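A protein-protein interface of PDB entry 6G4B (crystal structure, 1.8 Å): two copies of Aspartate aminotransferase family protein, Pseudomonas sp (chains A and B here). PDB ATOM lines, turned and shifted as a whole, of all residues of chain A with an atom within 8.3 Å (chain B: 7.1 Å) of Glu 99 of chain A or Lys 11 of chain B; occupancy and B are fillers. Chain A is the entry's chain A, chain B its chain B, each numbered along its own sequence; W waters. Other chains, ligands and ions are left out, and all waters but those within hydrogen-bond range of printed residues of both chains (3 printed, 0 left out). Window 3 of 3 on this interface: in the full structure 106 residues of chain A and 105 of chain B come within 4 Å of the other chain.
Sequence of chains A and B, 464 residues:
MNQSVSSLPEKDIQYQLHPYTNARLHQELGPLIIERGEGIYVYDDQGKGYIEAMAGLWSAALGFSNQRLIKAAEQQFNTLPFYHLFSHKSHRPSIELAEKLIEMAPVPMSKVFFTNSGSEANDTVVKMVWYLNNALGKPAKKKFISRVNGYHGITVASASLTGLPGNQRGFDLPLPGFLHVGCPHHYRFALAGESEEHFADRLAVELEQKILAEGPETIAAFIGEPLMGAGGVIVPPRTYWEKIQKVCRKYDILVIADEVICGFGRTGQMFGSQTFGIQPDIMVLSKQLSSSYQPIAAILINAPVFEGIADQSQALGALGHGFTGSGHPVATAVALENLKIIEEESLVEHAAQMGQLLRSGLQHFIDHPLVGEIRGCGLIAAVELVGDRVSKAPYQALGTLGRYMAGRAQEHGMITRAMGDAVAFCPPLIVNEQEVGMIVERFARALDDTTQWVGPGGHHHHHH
Among the printed residues, pairs that only touch across the chains: Phe 114 of chain A with Gln 16 of chain B, Lys 111 of chain A with Tyr 15 of chain B, Ile 95 of chain A with Gln 16 of chain B, Ile 95 of chain A with Asp 12 of chain B, Ile 95 of chain A with Lys 11 of chain B, Glu 99 of chain A with Tyr 15 of chain B, Lys 111 of chain A with Ile 13 of chain B, Ala 98 of chain A with Gln 16 of chain B, Arg 92 of chain A with Leu 8 of chain B, Ile 102 of chain A with Tyr 15 of chain B, Ile 95 of chain A with Leu 8 of chain B, Val 112 of chain A with Gln 16 of chain B, Ala 98 of chain A with Tyr 15 of chain B and Lys 111 of chain A with Gln 16 of chain B.
No position is printed for both chains.
Of the 22 pairs that touch across the chains among the printed residues, none has its exchanged pair printed and touching as well.
The side-chain carboxylate of Glu 96 of chain A is in salt-bridge range of the guanidinium group of Arg 92 of chain A (2.9 Å).
OG of Ser 110 of chain A is in hydrogen-bond range of NZ of Lys 111 of chain A, 3.0 Å away.
The side-chain carboxylate (OD1) of Asp 12 of chain B lies within hydrogen-bond range of the side-chain amide nitrogen (NE2) of Gln 16 of chain B (3.0 Å).
Printed residues of chain B within 4 Å of Ile 95 of chain A: Leu 8 (3.7 Å), Lys 11 (3.5 Å), Asp 12 (3.5 Å) and Gln 16 (3.5 Å).
Of the printed residues of chain B, Ser 110 of chain A touches Gln 14.
Printed residues of chain B within 4 Å of Phe 114 of chain A: Gln 16 (3.3 Å).
Pro 9 of chain B touches none of the printed residues of chain A.
Lys 11 of chain B touches two residues of chain A.
The nearest residue of chain B that does not touch Glu 99 of chain A is Ser 6 of chain B (5.8 Å).
The nearest residue of chain A that does not touch Lys 11 of chain B is Glu 96 of chain A (5.5 Å).
Of the 21 printed residues of chain A, 12 touch a printed residue of chain B.
Hydrophobic or aromatic side chains of chain B within 4 Å of the printed part of chain A: Leu 8 and Tyr 15.
Among the printed residues, Asp or Glu carboxylates within 4 Å of a Lys or Arg side-chain nitrogen of the other chain: Glu 99 of chain A with Lys 11 of chain B.
Water W1 lies within hydrogen-bond range of OH of Tyr 15 of chain B (2.6 Å) and OE2 of Glu 99 of chain A (2.8 Å).
Water W2 bridges the backbone carbonyl oxygen of Ser 110 of chain A and the backbone carbonyl oxygen of Gln 14 of chain B.
Water W3 bridges OE1 of Gln 16 of chain B and O of Val 112 of chain A.
NZ of Lys 111 of chain A sits at hydrogen-bond distance from O of Gln 14 of chain B (2.8 Å).
The backbone NH (N) of Val 112 of chain A sits at hydrogen-bond distance from the backbone carbonyl oxygen (O) of Tyr 15 of chain B, at 2.9 Å.
OD1 of Asp 12 of chain B sits at hydrogen-bond distance from OG of Ser 90 of chain A (2.7 Å).
The side-chain hydroxyl (OG) of Ser 94 of chain A is in hydrogen-bond range of the side-chain amide nitrogen (NE2) of Gln 16 of chain B (3.0 Å).
The side-chain carboxylate of Glu 99 of chain A is in salt-bridge range of the side-chain amino group of Lys 11 of chain B (2.9 Å).
The backbone carbonyl oxygen (O) of Gln 14 of chain B sits close to the backbone carbonyl oxygen (O) of Ser 110 of chain A, at 3.2 Å.
The side-chain amide nitrogen of Gln 16 of chain B is in hydrogen-bond range of the side-chain hydroxyl of Ser 90 of chain A, 3.3 Å away.
OE2 of Glu 103 of chain A is in hydrogen-bond range of OH of Tyr 15 of chain B, 2.8 Å away.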
ATOM      1  N   SER A  90      10.406   1.435  19.155  1.00  0.00           N
ATOM      2  CA  SER A  90      10.201   0.053  19.553  1.00  0.00           C
ATOM      3  C   SER A  90      10.736  -0.199  20.952  1.00  0.00           C
ATOM      4  O   SER A  90      11.305   0.696  21.584  1.00  0.00           O
ATOM      5  CB  SER A  90      10.847  -0.905  18.542  1.00  0.00           C
ATOM      6  OG  SER A  90      10.213  -2.175  18.604  1.00  0.00           O
ATOM      7  N   ARG A  92      12.010  -3.829  23.693  1.00  0.00           N
ATOM      8  CA  ARG A  92      12.425  -5.235  23.707  1.00  0.00           C
ATOM      9  C   ARG A  92      11.281  -6.242  23.841  1.00  0.00           C
ATOM     10  O   ARG A  92      11.277  -7.241  23.131  1.00  0.00           O
ATOM     11  CB  ARG A  92      13.486  -5.480  24.789  1.00  0.00           C
ATOM     12  CG  ARG A  92      13.926  -6.934  24.928  1.00  0.00           C
ATOM     13  CD  ARG A  92      14.831  -7.131  26.134  1.00  0.00           C
ATOM     14  NE  ARG A  92      16.111  -6.474  25.911  1.00  0.00           N
ATOM     15  CZ  ARG A  92      17.122  -6.995  25.212  1.00  0.00           C
ATOM     16  NH1 ARG A  92      17.017  -8.200  24.653  1.00  0.00           N
ATOM     17  NH2 ARG A  92      18.252  -6.303  25.057  1.00  0.00           N
ATOM     18  N   PRO A  93      10.335  -6.019  24.781  1.00  0.00           N
ATOM     19  CA  PRO A  93       9.319  -7.076  24.959  1.00  0.00           C
ATOM     20  C   PRO A  93       8.446  -7.289  23.719  1.00  0.00           C
ATOM     21  O   PRO A  93       8.133  -8.440  23.397  1.00  0.00           O
ATOM     22  CB  PRO A  93       8.483  -6.612  26.156  1.00  0.00           C
ATOM     23  CG  PRO A  93       9.148  -5.413  26.712  1.00  0.00           C
ATOM     24  CD  PRO A  93      10.299  -5.003  25.844  1.00  0.00           C
ATOM     25  N   SER A  94       8.107  -6.217  22.989  1.00  0.00           N
ATOM     26  CA  SER A  94       7.326  -6.397  21.750  1.00  0.00           C
ATOM     27  C   SER A  94       8.151  -7.178  20.718  1.00  0.00           C
ATOM     28  O   SER A  94       7.638  -8.062  20.040  1.00  0.00           O
ATOM     29  CB  SER A  94       6.858  -5.082  21.148  1.00  0.00           C
ATOM     30  OG  SER A  94       7.946  -4.255  20.758  1.00  0.00           O
ATOM     31  N   ILE A  95       9.431  -6.856  20.630  1.00  0.00           N
ATOM     32  CA  ILE A  95      10.317  -7.517  19.661  1.00  0.00           C
ATOM     33  C   ILE A  95      10.457  -9.003  19.966  1.00  0.00           C
ATOM     34  O   ILE A  95      10.318  -9.839  19.078  1.00  0.00           O
ATOM     35  CB  ILE A  95      11.699  -6.843  19.629  1.00  0.00           C
ATOM     36  CG1 ILE A  95      11.572  -5.391  19.145  1.00  0.00           C
ATOM     37  CG2 ILE A  95      12.651  -7.600  18.705  1.00  0.00           C
ATOM     38  CD1 ILE A  95      12.806  -4.555  19.427  1.00  0.00           C
ATOM     39  N   GLU A  96      10.726  -9.332  21.223  1.00  0.00           N
ATOM     40  CA  GLU A  96      10.951 -10.719  21.602  1.00  0.00           C
ATOM     41  C   GLU A  96       9.662 -11.542  21.519  1.00  0.00           C
ATOM     42  O   GLU A  96       9.698 -12.708  21.144  1.00  0.00           O
ATOM     43  CB  GLU A  96      11.610 -10.820  22.981  1.00  0.00           C
ATOM     44  CG  GLU A  96      13.027 -10.242  22.990  1.00  0.00           C
ATOM     45  CD  GLU A  96      13.760 -10.413  24.312  1.00  0.00           C
ATOM     46  OE1 GLU A  96      13.130 -10.758  25.324  1.00  0.00           O
ATOM     47  OE2 GLU A  96      14.984 -10.175  24.335  1.00  0.00           O
ATOM     48  N   LEU A  97       8.523 -10.938  21.844  1.00  0.00           N
ATOM     49  CA  LEU A  97       7.268 -11.654  21.708  1.00  0.00           C
ATOM     50  C   LEU A  97       6.956 -11.898  20.229  1.00  0.00           C
ATOM     51  O   LEU A  97       6.506 -12.995  19.851  1.00  0.00           O
ATOM     52  CB  LEU A  97       6.139 -10.884  22.392  1.00  0.00           C
ATOM     53  CG  LEU A  97       4.746 -11.537  22.291  1.00  0.00           C
ATOM     54  CD1 LEU A  97       4.742 -12.938  22.899  1.00  0.00           C
ATOM     55  CD2 LEU A  97       3.735 -10.657  22.985  1.00  0.00           C
ATOM     56  N   ALA A  98       7.194 -10.885  19.387  1.00  0.00           N
ATOM     57  CA  ALA A  98       6.922 -11.028  17.956  1.00  0.00           C
ATOM     58  C   ALA A  98       7.768 -12.153  17.354  1.00  0.00           C
ATOM     59  O   ALA A  98       7.259 -13.005  16.624  1.00  0.00           O
ATOM     60  CB  ALA A  98       7.167  -9.714  17.227  1.00  0.00           C
ATOM     61  N   GLU A  99       9.045 -12.182  17.710  1.00  0.00           N
ATOM     62  CA  GLU A  99       9.935 -13.279  17.327  1.00  0.00           C
ATOM     63  C   GLU A  99       9.376 -14.639  17.742  1.00  0.00           C
ATOM     64  O   GLU A  99       9.327 -15.589  16.941  1.00  0.00           O
ATOM     65  CB  GLU A  99      11.306 -13.095  17.978  1.00  0.00           C
ATOM     66  CG  GLU A  99      12.217 -14.317  17.855  1.00  0.00           C
ATOM     67  CD  GLU A  99      13.587 -14.119  18.494  1.00  0.00           C
ATOM     68  OE1 GLU A  99      13.664 -13.608  19.638  1.00  0.00           O
ATOM     69  OE2 GLU A  99      14.585 -14.484  17.848  1.00  0.00           O
ATOM     70  N   LYS A 100       8.969 -14.745  19.003  1.00  0.00           N
ATOM     71  CA  LYS A 100       8.498 -16.020  19.526  1.00  0.00           C
ATOM     72  C   LYS A 100       7.233 -16.484  18.803  1.00  0.00           C
ATOM     73  O   LYS A 100       7.103 -17.655  18.452  1.00  0.00           O
ATOM     74  CB  LYS A 100       8.224 -15.919  21.010  1.00  0.00           C
ATOM     75  CG  LYS A 100       7.996 -17.280  21.658  1.00  0.00           C
ATOM     76  CD  LYS A 100       7.827 -17.145  23.157  1.00  0.00           C
ATOM     77  CE  LYS A 100       8.240 -18.379  23.968  1.00  0.00           C
ATOM     78  NZ  LYS A 100       9.006 -19.471  23.289  1.00  0.00           N
ATOM     79  N   LEU A 101       6.302 -15.563  18.605  1.00  0.00           N
ATOM     80  CA  LEU A 101       5.061 -15.875  17.898  1.00  0.00           C
ATOM     81  C   LEU A 101       5.316 -16.348  16.464  1.00  0.00           C
ATOM     82  O   LEU A 101       4.741 -17.346  16.034  1.00  0.00           O
ATOM     83  CB  LEU A 101       4.112 -14.668  17.903  1.00  0.00           C
ATOM     84  CG  LEU A 101       3.508 -14.341  19.259  1.00  0.00           C
ATOM     85  CD1 LEU A 101       2.801 -12.987  19.232  1.00  0.00           C
ATOM     86  CD2 LEU A 101       2.542 -15.437  19.712  1.00  0.00           C
ATOM     87  N   ILE A 102       6.188 -15.649  15.741  1.00  0.00           N
ATOM     88  CA  ILE A 102       6.502 -16.049  14.365  1.00  0.00           C
ATOM     89  C   ILE A 102       7.174 -17.413  14.364  1.00  0.00           C
ATOM     90  O   ILE A 102       6.831 -18.286  13.554  1.00  0.00           O
ATOM     91  CB  ILE A 102       7.373 -14.997  13.643  1.00  0.00           C
ATOM     92  CG1 ILE A 102       6.587 -13.685  13.420  1.00  0.00           C
ATOM     93  CG2 ILE A 102       7.939 -15.545  12.331  1.00  0.00           C
ATOM     94  CD1 ILE A 102       5.369 -13.783  12.518  1.00  0.00           C
ATOM     95  N   GLU A 103       8.100 -17.626  15.283  1.00  0.00           N
ATOM     96  CA  GLU A 103       8.839 -18.866  15.255  1.00  0.00           C
ATOM     97  C   GLU A 103       8.000 -20.051  15.722  1.00  0.00           C
ATOM     98  O   GLU A 103       8.261 -21.162  15.305  1.00  0.00           O
ATOM     99  CB  GLU A 103      10.178 -18.720  15.984  1.00  0.00           C
ATOM    100  CG  GLU A 103      11.112 -17.703  15.286  1.00  0.00           C
ATOM    101  CD  GLU A 103      11.524 -18.075  13.848  1.00  0.00           C
ATOM    102  OE1 GLU A 103      11.524 -19.274  13.490  1.00  0.00           O
ATOM    103  OE2 GLU A 103      11.884 -17.170  13.064  1.00  0.00           O
ATOM    104  N   MET A 104       6.947 -19.819  16.500  1.00  0.00           N
ATOM    105  CA  MET A 104       6.074 -20.924  16.897  1.00  0.00           C
ATOM    106  C   MET A 104       4.870 -21.145  15.961  1.00  0.00           C
ATOM    107  O   MET A 104       4.119 -22.088  16.156  1.00  0.00           O
ATOM    108  CB  MET A 104       5.634 -20.747  18.364  1.00  0.00           C
ATOM    109  CG  MET A 104       4.536 -19.766  18.613  1.00  0.00           C
ATOM    110  SD  MET A 104       4.422 -19.403  20.413  1.00  0.00           S
ATOM    111  CE  MET A 104       3.636 -20.941  20.966  1.00  0.00           C
ATOM    112  N   ALA A 105       4.696 -20.292  14.951  1.00  0.00           N
ATOM    113  CA  ALA A 105       3.522 -20.358  14.073  1.00  0.00           C
ATOM    114  C   ALA A 105       3.466 -21.696  13.344  1.00  0.00           C
ATOM    115  O   ALA A 105       4.498 -22.238  12.960  1.00  0.00           O
ATOM    116  CB  ALA A 105       3.522 -19.225  13.070  1.00  0.00           C
ATOM    117  N   SER A 110       5.114 -13.984   8.446  1.00  0.00           N
ATOM    118  CA  SER A 110       6.058 -12.918   8.170  1.00  0.00           C
ATOM    119  C   SER A 110       6.133 -11.866   9.283  1.00  0.00           C
ATOM    120  O   SER A 110       7.236 -11.546   9.765  1.00  0.00           O
ATOM    121  CB  SER A 110       5.731 -12.255   6.831  1.00  0.00           C
ATOM    122  OG  SER A 110       6.609 -11.173   6.583  1.00  0.00           O
ATOM    123  N   LYS A 111       4.989 -11.346   9.716  1.00  0.00           N
ATOM    124  CA  LYS A 111       4.979 -10.246  10.684  1.00  0.00           C
ATOM    125  C   LYS A 111       3.855 -10.371  11.701  1.00  0.00           C
ATOM    126  O   LYS A 111       2.854 -11.025  11.428  1.00  0.00           O
ATOM    127  CB  LYS A 111       4.807  -8.902   9.971  1.00  0.00           C
ATOM    128  CG  LYS A 111       5.873  -8.567   8.932  1.00  0.00           C
ATOM    129  CD  LYS A 111       7.222  -8.227   9.557  1.00  0.00           C
ATOM    130  CE  LYS A 111       8.312  -8.159   8.480  1.00  0.00           C
ATOM    131  NZ  LYS A 111       8.708  -9.511   7.960  1.00  0.00           N
ATOM    132  N   VAL A 112       4.072  -9.753  12.865  1.00  0.00           N
ATOM    133  CA  VAL A 112       3.076  -9.607  13.916  1.00  0.00           C
ATOM    134  C   VAL A 112       2.651  -8.145  14.052  1.00  0.00           C
ATOM    135  O   VAL A 112       3.496  -7.233  14.029  1.00  0.00           O
ATOM    136  CB  VAL A 112       3.658 -10.005  15.274  1.00  0.00           C
ATOM    137  CG1 VAL A 112       2.596  -9.924  16.363  1.00  0.00           C
ATOM    138  CG2 VAL A 112       4.252 -11.400  15.212  1.00  0.00           C
ATOM    139  N   PHE A 114       0.256  -5.983  16.809  1.00  0.00           N
ATOM    140  CA  PHE A 114      -0.354  -6.130  18.133  1.00  0.00           C
ATOM    141  C   PHE A 114      -1.529  -5.189  18.323  1.00  0.00           C
ATOM    142  O   PHE A 114      -1.521  -4.036  17.848  1.00  0.00           O
ATOM    143  CB  PHE A 114       0.667  -5.851  19.250  1.00  0.00           C
ATOM    144  CG  PHE A 114       1.749  -6.899  19.384  1.00  0.00           C
ATOM    145  CD1 PHE A 114       1.438  -8.170  19.832  1.00  0.00           C
ATOM    146  CD2 PHE A 114       3.069  -6.600  19.091  1.00  0.00           C
ATOM    147  CE1 PHE A 114       2.410  -9.135  19.990  1.00  0.00           C
ATOM    148  CE2 PHE A 114       4.059  -7.566  19.227  1.00  0.00           C
ATOM    149  CZ  PHE A 114       3.736  -8.835  19.694  1.00  0.00           C
ATOM    150  N   LEU A 336       4.956 -12.869  26.852  1.00  0.00           N
ATOM    151  CA  LEU A 336       6.178 -13.603  26.548  1.00  0.00           C
ATOM    152  C   LEU A 336       6.455 -14.659  27.628  1.00  0.00           C
ATOM    153  O   LEU A 336       6.756 -15.816  27.315  1.00  0.00           O
ATOM    154  CB  LEU A 336       7.323 -12.639  26.376  1.00  0.00           C
ATOM    155  CG  LEU A 336       8.697 -13.207  26.095  1.00  0.00           C
ATOM    156  CD1 LEU A 336       8.721 -13.961  24.768  1.00  0.00           C
ATOM    157  CD2 LEU A 336       9.695 -12.064  26.083  1.00  0.00           C
ATOM    158  N   LEU A 339       3.954 -17.637  27.465  1.00  0.00           N
ATOM    159  CA  LEU A 339       4.275 -18.640  26.450  1.00  0.00           C
ATOM    160  C   LEU A 339       5.458 -19.527  26.851  1.00  0.00           C
ATOM    161  O   LEU A 339       5.426 -20.742  26.655  1.00  0.00           O
ATOM    162  CB  LEU A 339       4.521 -17.966  25.091  1.00  0.00           C
ATOM    163  CG  LEU A 339       3.334 -17.161  24.535  1.00  0.00           C
ATOM    164  CD1 LEU A 339       3.672 -16.624  23.143  1.00  0.00           C
ATOM    165  CD2 LEU A 339       2.074 -17.984  24.488  1.00  0.00           C
ATOM    166  N   SER B   6      21.641 -12.609  15.754  1.00  0.00           N
ATOM    167  CA  SER B   6      20.568 -11.616  15.400  1.00  0.00           C
ATOM    168  C   SER B   6      20.431 -10.528  16.472  1.00  0.00           C
ATOM    169  O   SER B   6      20.102 -10.810  17.624  1.00  0.00           O
ATOM    170  CB  SER B   6      19.212 -12.305  15.185  1.00  0.00           C
ATOM    171  OG  SER B   6      18.737 -12.122  13.863  1.00  0.00           O
ATOM    172  N   SER B   7      20.679  -9.281  16.086  1.00  0.00           N
ATOM    173  CA  SER B   7      20.536  -8.146  17.004  1.00  0.00           C
ATOM    174  C   SER B   7      19.065  -7.804  17.253  1.00  0.00           C
ATOM    175  O   SER B   7      18.189  -8.235  16.515  1.00  0.00           O
ATOM    176  CB  SER B   7      21.275  -6.919  16.453  1.00  0.00           C
ATOM    177  OG  SER B   7      20.561  -6.327  15.370  1.00  0.00           O
ATOM    178  N   LEU B   8      18.811  -7.004  18.283  1.00  0.00           N
ATOM    179  CA  LEU B   8      17.457  -6.626  18.629  1.00  0.00           C
ATOM    180  C   LEU B   8      16.802  -5.800  17.508  1.00  0.00           C
ATOM    181  O   LEU B   8      15.662  -6.079  17.135  1.00  0.00           O
ATOM    182  CB  LEU B   8      17.423  -5.879  19.964  1.00  0.00           C
ATOM    183  CG  LEU B   8      16.130  -5.972  20.775  1.00  0.00           C
ATOM    184  CD1 LEU B   8      15.698  -7.411  21.027  1.00  0.00           C
ATOM    185  CD2 LEU B   8      16.324  -5.239  22.093  1.00  0.00           C
ATOM    186  N   PRO B   9      17.529  -4.810  16.939  1.00  0.00           N
ATOM    187  CA  PRO B   9      16.944  -4.095  15.792  1.00  0.00           C
ATOM    188  C   PRO B   9      16.659  -5.011  14.598  1.00  0.00           C
ATOM    189  O   PRO B   9      15.666  -4.809  13.901  1.00  0.00           O
ATOM    190  CB  PRO B   9      18.022  -3.052  15.418  1.00  0.00           C
ATOM    191  CG  PRO B   9      18.894  -2.929  16.625  1.00  0.00           C
ATOM    192  CD  PRO B   9      18.819  -4.229  17.362  1.00  0.00           C
ATOM    193  N   GLU B  10      17.540  -5.978  14.345  1.00  0.00           N
ATOM    194  CA  GLU B  10      17.319  -6.920  13.255  1.00  0.00           C
ATOM    195  C   GLU B  10      16.052  -7.749  13.484  1.00  0.00           C
ATOM    196  O   GLU B  10      15.277  -7.967  12.558  1.00  0.00           O
ATOM    197  CB  GLU B  10      18.528  -7.829  13.062  1.00  0.00           C
ATOM    198  CG  GLU B  10      19.674  -7.094  12.389  1.00  0.00           C
ATOM    199  CD  GLU B  10      20.995  -7.840  12.417  1.00  0.00           C
ATOM    200  OE1 GLU B  10      21.139  -8.850  13.137  1.00  0.00           O
ATOM    201  OE2 GLU B  10      21.908  -7.379  11.711  1.00  0.00           O
ATOM    202  N   LYS B  11      15.847  -8.187  14.718  1.00  0.00           N
ATOM    203  CA  LYS B  11      14.633  -8.922  15.074  1.00  0.00           C
ATOM    204  C   LYS B  11      13.392  -8.060  14.902  1.00  0.00           C
ATOM    205  O   LYS B  11      12.372  -8.529  14.399  1.00  0.00           O
ATOM    206  CB  LYS B  11      14.709  -9.424  16.518  1.00  0.00           C
ATOM    207  CG  LYS B  11      15.763 -10.510  16.747  1.00  0.00           C
ATOM    208  CD  LYS B  11      15.800 -10.883  18.226  1.00  0.00           C
ATOM    209  CE  LYS B  11      16.992 -11.696  18.652  1.00  0.00           C
ATOM    210  NZ  LYS B  11      17.064 -12.939  17.864  1.00  0.00           N
ATOM    211  N   ASP B  12      13.492  -6.787  15.292  1.00  0.00           N
ATOM    212  CA  ASP B  12      12.354  -5.878  15.148  1.00  0.00           C
ATOM    213  C   ASP B  12      11.955  -5.775  13.682  1.00  0.00           C
ATOM    214  O   ASP B  12      10.775  -5.867  13.340  1.00  0.00           O
ATOM    215  CB  ASP B  12      12.696  -4.493  15.691  1.00  0.00           C
ATOM    216  CG  ASP B  12      11.547  -3.519  15.525  1.00  0.00           C
ATOM    217  OD1 ASP B  12      10.559  -3.611  16.299  1.00  0.00           O
ATOM    218  OD2 ASP B  12      11.626  -2.681  14.610  1.00  0.00           O
ATOM    219  N   ILE B  13      12.948  -5.545  12.823  1.00  0.00           N
ATOM    220  CA  ILE B  13      12.714  -5.402  11.387  1.00  0.00           C
ATOM    221  C   ILE B  13      12.134  -6.690  10.802  1.00  0.00           C
ATOM    222  O   ILE B  13      11.254  -6.631   9.945  1.00  0.00           O
ATOM    223  CB  ILE B  13      14.028  -5.034  10.643  1.00  0.00           C
ATOM    224  CG1 ILE B  13      14.422  -3.575  10.934  1.00  0.00           C
ATOM    225  CG2 ILE B  13      13.898  -5.265   9.142  1.00  0.00           C
ATOM    226  CD1 ILE B  13      15.850  -3.251  10.519  1.00  0.00           C
ATOM    227  N   GLN B  14      12.634  -7.837  11.263  1.00  0.00           N
ATOM    228  CA  GLN B  14      12.204  -9.131  10.746  1.00  0.00           C
ATOM    229  C   GLN B  14      10.756  -9.495  11.127  1.00  0.00           C
ATOM    230  O   GLN B  14      10.051 -10.133  10.331  1.00  0.00           O
ATOM    231  CB  GLN B  14      13.134 -10.248  11.239  1.00  0.00           C
ATOM    232  CG  GLN B  14      12.903 -11.599  10.572  1.00  0.00           C
ATOM    233  CD  GLN B  14      13.157 -11.540   9.065  1.00  0.00           C
ATOM    234  OE1 GLN B  14      14.214 -11.072   8.627  1.00  0.00           O
ATOM    235  NE2 GLN B  14      12.189 -12.006   8.265  1.00  0.00           N
ATOM    236  N   TYR B  15      10.340  -9.114  12.327  1.00  0.00           N
ATOM    237  CA  TYR B  15       9.114  -9.696  12.904  1.00  0.00           C
ATOM    238  C   TYR B  15       7.961  -8.757  13.162  1.00  0.00           C
ATOM    239  O   TYR B  15       6.840  -9.232  13.329  1.00  0.00           O
ATOM    240  CB  TYR B  15       9.441 -10.398  14.221  1.00  0.00           C
ATOM    241  CG  TYR B  15      10.446 -11.529  14.058  1.00  0.00           C
ATOM    242  CD1 TYR B  15      10.171 -12.608  13.219  1.00  0.00           C
ATOM    243  CD2 TYR B  15      11.655 -11.532  14.756  1.00  0.00           C
ATOM    244  CE1 TYR B  15      11.060 -13.654  13.069  1.00  0.00           C
ATOM    245  CE2 TYR B  15      12.553 -12.574  14.621  1.00  0.00           C
ATOM    246  CZ  TYR B  15      12.245 -13.638  13.778  1.00  0.00           C
ATOM    247  OH  TYR B  15      13.118 -14.684  13.621  1.00  0.00           O
ATOM    248  N   GLN B  16       8.209  -7.456  13.266  1.00  0.00           N
ATOM    249  CA  GLN B  16       7.147  -6.528  13.673  1.00  0.00           C
ATOM    250  C   GLN B  16       6.669  -5.624  12.559  1.00  0.00           C
ATOM    251  O   GLN B  16       7.471  -4.967  11.905  1.00  0.00           O
ATOM    252  CB  GLN B  16       7.599  -5.623  14.815  1.00  0.00           C
ATOM    253  CG  GLN B  16       7.910  -6.353  16.085  1.00  0.00           C
ATOM    254  CD  GLN B  16       7.462  -5.566  17.293  1.00  0.00           C
ATOM    255  OE1 GLN B  16       6.317  -5.670  17.717  1.00  0.00           O
ATOM    256  NE2 GLN B  16       8.371  -4.812  17.877  1.00  0.00           N
HETATM  257  O   HOH W   1      15.212 -15.000  15.193  1.00  0.00           O
HETATM  258  O   HOH W   2       9.507 -12.894   9.290  1.00  0.00           O
HETATM  259  O   HOH W   3       4.301  -5.282  15.977  1.00  0.00           O
